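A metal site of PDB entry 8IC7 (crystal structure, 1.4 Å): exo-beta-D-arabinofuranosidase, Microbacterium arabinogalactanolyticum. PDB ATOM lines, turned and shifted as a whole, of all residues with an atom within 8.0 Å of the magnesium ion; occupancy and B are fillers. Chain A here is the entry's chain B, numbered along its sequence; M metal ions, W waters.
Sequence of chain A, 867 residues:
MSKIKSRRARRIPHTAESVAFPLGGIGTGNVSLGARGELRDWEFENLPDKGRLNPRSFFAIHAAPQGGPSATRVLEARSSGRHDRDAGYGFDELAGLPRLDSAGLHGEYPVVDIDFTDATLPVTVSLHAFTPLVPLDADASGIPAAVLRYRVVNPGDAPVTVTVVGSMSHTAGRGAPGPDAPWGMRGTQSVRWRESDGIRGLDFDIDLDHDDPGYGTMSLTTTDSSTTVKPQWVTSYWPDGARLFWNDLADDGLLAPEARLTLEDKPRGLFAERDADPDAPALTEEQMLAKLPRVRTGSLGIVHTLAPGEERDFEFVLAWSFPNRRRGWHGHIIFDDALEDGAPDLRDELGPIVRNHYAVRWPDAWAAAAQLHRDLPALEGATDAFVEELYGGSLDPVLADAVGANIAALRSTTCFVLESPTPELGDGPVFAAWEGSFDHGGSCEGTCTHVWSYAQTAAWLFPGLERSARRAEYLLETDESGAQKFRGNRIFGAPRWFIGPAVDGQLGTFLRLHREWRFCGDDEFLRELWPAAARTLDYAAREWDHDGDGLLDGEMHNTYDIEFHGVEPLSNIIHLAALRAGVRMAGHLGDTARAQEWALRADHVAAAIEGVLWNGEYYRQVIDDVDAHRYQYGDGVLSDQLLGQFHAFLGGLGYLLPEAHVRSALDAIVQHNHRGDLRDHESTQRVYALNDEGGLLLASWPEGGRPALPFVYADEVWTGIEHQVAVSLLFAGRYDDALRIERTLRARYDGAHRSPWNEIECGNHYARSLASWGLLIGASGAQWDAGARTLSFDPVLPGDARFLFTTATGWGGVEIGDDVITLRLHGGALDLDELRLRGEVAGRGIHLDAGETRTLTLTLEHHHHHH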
ATOM      1  N   THR A 228       7.718 -12.010  -8.866  1.00  0.00           N
ATOM      2  CA  THR A 228       6.273 -12.179  -8.889  1.00  0.00           C
ATOM      3  C   THR A 228       5.794 -11.364 -10.089  1.00  0.00           C
ATOM      4  O   THR A 228       6.285 -10.258 -10.316  1.00  0.00           O
ATOM      5  CB  THR A 228       5.603 -11.705  -7.586  1.00  0.00           C
ATOM      6  OG1 THR A 228       4.224 -12.107  -7.577  1.00  0.00           O
ATOM      7  CG2 THR A 228       5.706 -10.211  -7.392  1.00  0.00           C
ATOM      8  N   LYS A 230       2.783 -10.333 -13.314  1.00  0.00           N
ATOM      9  CA  LYS A 230       1.558 -10.333 -14.087  1.00  0.00           C
ATOM     10  C   LYS A 230       1.959 -10.038 -15.529  1.00  0.00           C
ATOM     11  O   LYS A 230       2.128  -8.860 -15.907  1.00  0.00           O
ATOM     12  CB  LYS A 230       0.566  -9.321 -13.537  1.00  0.00           C
ATOM     13  CG  LYS A 230      -0.748  -9.194 -14.294  1.00  0.00           C
ATOM     14  CD  LYS A 230      -1.725  -8.150 -13.734  1.00  0.00           C
ATOM     15  CE  LYS A 230      -2.134  -8.370 -12.289  1.00  0.00           C
ATOM     16  NZ  LYS A 230      -2.910  -9.612 -12.142  1.00  0.00           N
ATOM     17  N   LEU A 244      -7.384  -3.928 -11.798  1.00  0.00           N
ATOM     18  CA  LEU A 244      -7.071  -5.286 -11.382  1.00  0.00           C
ATOM     19  C   LEU A 244      -5.637  -5.414 -10.946  1.00  0.00           C
ATOM     20  O   LEU A 244      -5.339  -6.125  -9.970  1.00  0.00           O
ATOM     21  CB  LEU A 244      -7.377  -6.265 -12.513  1.00  0.00           C
ATOM     22  CG  LEU A 244      -8.845  -6.386 -12.915  1.00  0.00           C
ATOM     23  CD1 LEU A 244      -8.953  -7.299 -14.114  1.00  0.00           C
ATOM     24  CD2 LEU A 244      -9.660  -6.876 -11.745  1.00  0.00           C
ATOM     25  N   PHE A 245      -4.706  -4.706 -11.618  1.00  0.00           N
ATOM     26  CA  PHE A 245      -3.315  -4.686 -11.194  1.00  0.00           C
ATOM     27  C   PHE A 245      -3.145  -4.109  -9.789  1.00  0.00           C
ATOM     28  O   PHE A 245      -2.571  -4.755  -8.910  1.00  0.00           O
ATOM     29  CB  PHE A 245      -2.449  -3.869 -12.140  1.00  0.00           C
ATOM     30  CG  PHE A 245      -1.079  -3.563 -11.569  1.00  0.00           C
ATOM     31  CD1 PHE A 245      -0.099  -4.555 -11.521  1.00  0.00           C
ATOM     32  CD2 PHE A 245      -0.792  -2.335 -10.995  1.00  0.00           C
ATOM     33  CE1 PHE A 245       1.173  -4.259 -11.034  1.00  0.00           C
ATOM     34  CE2 PHE A 245       0.453  -2.067 -10.427  1.00  0.00           C
ATOM     35  CZ  PHE A 245       1.432  -3.042 -10.430  1.00  0.00           C
ATOM     36  N   TRP A 246      -3.721  -2.962  -9.497  1.00  0.00           N
ATOM     37  CA  TRP A 246      -3.600  -2.364  -8.177  1.00  0.00           C
ATOM     38  C   TRP A 246      -4.292  -3.225  -7.127  1.00  0.00           C
ATOM     39  O   TRP A 246      -3.774  -3.350  -6.023  1.00  0.00           O
ATOM     40  CB  TRP A 246      -4.137  -0.929  -8.153  1.00  0.00           C
ATOM     41  CG  TRP A 246      -3.662  -0.182  -6.939  1.00  0.00           C
ATOM     42  CD1 TRP A 246      -4.366   0.083  -5.790  1.00  0.00           C
ATOM     43  CD2 TRP A 246      -2.346   0.379  -6.727  1.00  0.00           C
ATOM     44  NE1 TRP A 246      -3.605   0.781  -4.899  1.00  0.00           N
ATOM     45  CE2 TRP A 246      -2.390   1.010  -5.455  1.00  0.00           C
ATOM     46  CE3 TRP A 246      -1.166   0.419  -7.476  1.00  0.00           C
ATOM     47  CZ2 TRP A 246      -1.313   1.720  -4.940  1.00  0.00           C
ATOM     48  CZ3 TRP A 246      -0.109   1.144  -6.964  1.00  0.00           C
ATOM     49  CH2 TRP A 246      -0.202   1.770  -5.716  1.00  0.00           C
ATOM     50  N   ASN A 247      -5.460  -3.795  -7.441  1.00  0.00           N
ATOM     51  CA  ASN A 247      -6.111  -4.682  -6.484  1.00  0.00           C
ATOM     52  C   ASN A 247      -5.122  -5.791  -6.114  1.00  0.00           C
ATOM     53  O   ASN A 247      -5.026  -6.221  -4.962  1.00  0.00           O
ATOM     54  CB  ASN A 247      -7.408  -5.302  -7.039  1.00  0.00           C
ATOM     55  CG  ASN A 247      -8.582  -4.359  -7.314  1.00  0.00           C
ATOM     56  OD1 ASN A 247      -8.561  -3.220  -6.907  1.00  0.00           O
ATOM     57  ND2 ASN A 247      -9.622  -4.811  -8.010  1.00  0.00           N
ATOM     58  N   ASP A 248      -4.519  -6.395  -7.151  1.00  0.00           N
ATOM     59  CA  ASP A 248      -3.637  -7.543  -6.983  1.00  0.00           C
ATOM     60  C   ASP A 248      -2.381  -7.198  -6.187  1.00  0.00           C
ATOM     61  O   ASP A 248      -1.942  -7.982  -5.328  1.00  0.00           O
ATOM     62  CB  ASP A 248      -3.230  -8.096  -8.351  1.00  0.00           C
ATOM     63  CG  ASP A 248      -2.562  -9.475  -8.394  1.00  0.00           C
ATOM     64  OD1 ASP A 248      -2.367 -10.084  -7.323  1.00  0.00           O
ATOM     65  OD2 ASP A 248      -2.288  -9.988  -9.514  1.00  0.00           O
ATOM     66  N   LEU A 249      -1.805  -6.004  -6.417  1.00  0.00           N
ATOM     67  CA  LEU A 249      -0.595  -5.608  -5.719  1.00  0.00           C
ATOM     68  C   LEU A 249      -0.884  -5.189  -4.284  1.00  0.00           C
ATOM     69  O   LEU A 249      -0.108  -5.524  -3.380  1.00  0.00           O
ATOM     70  CB  LEU A 249       0.034  -4.437  -6.467  1.00  0.00           C
ATOM     71  CG  LEU A 249       1.332  -3.919  -5.845  1.00  0.00           C
ATOM     72  CD1 LEU A 249       2.415  -4.973  -5.905  1.00  0.00           C
ATOM     73  CD2 LEU A 249       1.793  -2.642  -6.546  1.00  0.00           C
ATOM     74  N   ALA A 250      -1.940  -4.382  -4.083  1.00  0.00           N
ATOM     75  CA  ALA A 250      -2.171  -3.780  -2.774  1.00  0.00           C
ATOM     76  C   ALA A 250      -2.724  -4.829  -1.813  1.00  0.00           C
ATOM     77  O   ALA A 250      -2.606  -4.667  -0.591  1.00  0.00           O
ATOM     78  CB  ALA A 250      -3.075  -2.581  -2.898  1.00  0.00           C
ATOM     79  N   ASP A 251      -3.311  -5.909  -2.327  1.00  0.00           N
ATOM     80  CA  ASP A 251      -3.803  -6.998  -1.494  1.00  0.00           C
ATOM     81  C   ASP A 251      -2.654  -7.627  -0.703  1.00  0.00           C
ATOM     82  O   ASP A 251      -2.678  -7.629   0.532  1.00  0.00           O
ATOM     83  CB  ASP A 251      -4.519  -8.024  -2.377  1.00  0.00           C
ATOM     84  CG  ASP A 251      -4.884  -9.301  -1.655  1.00  0.00           C
ATOM     85  OD1 ASP A 251      -5.578  -9.171  -0.656  1.00  0.00           O
ATOM     86  OD2 ASP A 251      -4.429 -10.388  -2.063  1.00  0.00           O
ATOM     87  N   ASP A 252      -1.631  -8.125  -1.399  1.00  0.00           N
ATOM     88  CA  ASP A 252      -0.660  -9.021  -0.802  1.00  0.00           C
ATOM     89  C   ASP A 252       0.773  -8.748  -1.239  1.00  0.00           C
ATOM     90  O   ASP A 252       1.660  -9.496  -0.846  1.00  0.00           O
ATOM     91  CB  ASP A 252      -1.015 -10.495  -1.046  1.00  0.00           C
ATOM     92  CG  ASP A 252      -1.100 -10.901  -2.507  1.00  0.00           C
ATOM     93  OD1 ASP A 252      -1.058  -9.981  -3.391  1.00  0.00           O
ATOM     94  OD2 ASP A 252      -1.202 -12.092  -2.774  1.00  0.00           O
ATOM     95  N   GLY A 253       1.018  -7.768  -2.112  1.00  0.00           N
ATOM     96  CA  GLY A 253       2.346  -7.546  -2.648  1.00  0.00           C
ATOM     97  C   GLY A 253       2.822  -8.599  -3.637  1.00  0.00           C
ATOM     98  O   GLY A 253       3.984  -8.563  -4.065  1.00  0.00           O
ATOM     99  N   LEU A 254       1.937  -9.503  -4.078  1.00  0.00           N
ATOM    100  CA  LEU A 254       2.227 -10.518  -5.069  1.00  0.00           C
ATOM    101  C   LEU A 254       1.273 -10.323  -6.259  1.00  0.00           C
ATOM    102  O   LEU A 254       0.186  -9.731  -6.098  1.00  0.00           O
ATOM    103  CB  LEU A 254       2.074 -11.913  -4.447  1.00  0.00           C
ATOM    104  CG  LEU A 254       2.989 -12.161  -3.234  1.00  0.00           C
ATOM    105  CD1 LEU A 254       2.747 -13.552  -2.703  1.00  0.00           C
ATOM    106  CD2 LEU A 254       4.467 -12.002  -3.596  1.00  0.00           C
ATOM    107  N   LEU A 255       1.665 -10.887  -7.402  1.00  0.00           N
ATOM    108  CA  LEU A 255       0.927 -10.759  -8.643  1.00  0.00           C
ATOM    109  C   LEU A 255       0.697 -12.127  -9.232  1.00  0.00           C
ATOM    110  O   LEU A 255       1.444 -13.074  -8.972  1.00  0.00           O
ATOM    111  CB  LEU A 255       1.765  -9.910  -9.598  1.00  0.00           C
ATOM    112  CG  LEU A 255       2.080  -8.496  -9.109  1.00  0.00           C
ATOM    113  CD1 LEU A 255       2.986  -7.852 -10.155  1.00  0.00           C
ATOM    114  CD2 LEU A 255       0.843  -7.650  -8.881  1.00  0.00           C
ATOM    115  N   ALA A 256      -0.340 -12.208 -10.063  1.00  0.00           N
ATOM    116  CA  ALA A 256      -0.608 -13.432 -10.785  1.00  0.00           C
ATOM    117  C   ALA A 256      -0.904 -13.073 -12.230  1.00  0.00           C
ATOM    118  O   ALA A 256      -1.454 -12.004 -12.487  1.00  0.00           O
ATOM    119  CB  ALA A 256      -1.729 -14.178 -10.140  1.00  0.00           C
HETATM  120 MG    MG M   1      -1.736 -10.040  -5.386  1.00  0.00          MG
HETATM  121  O   HOH W   1      -1.326 -12.140  -5.405  1.00  0.00           O
HETATM  122  O   HOH W   2      -3.654 -10.378  -4.634  1.00  0.00           O
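Three residues have an atom within 4 Å of the magnesium ion: Asp 248, Asp 252 and Leu 254.
The nearest printed residue that does not touch the magnesium ion is Leu 255 (4.04 Å).
The magnesium ion is bound by the side-chain carboxylate (OD1) of Asp 248 (2.0 Å), the backbone carbonyl oxygen (O) of Asp 248 (2.1 Å), the backbone carbonyl oxygen (O) of Leu 254 (2.1 Å), water W2 (2.1 Å), the side-chain carboxylate (OD1) of Asp 252 (2.1 Å) and water W1 (2.1 Å).
The magnesium ion has six donor atoms within binding distance.
The side-chain carboxylate (OD2) of Asp 248 lies within hydrogen-bond range of the backbone NH (N) of Ala 256.
OD2 of Asp 248 is in salt-bridge range of NZ of Lys 230 (2.7 Å).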
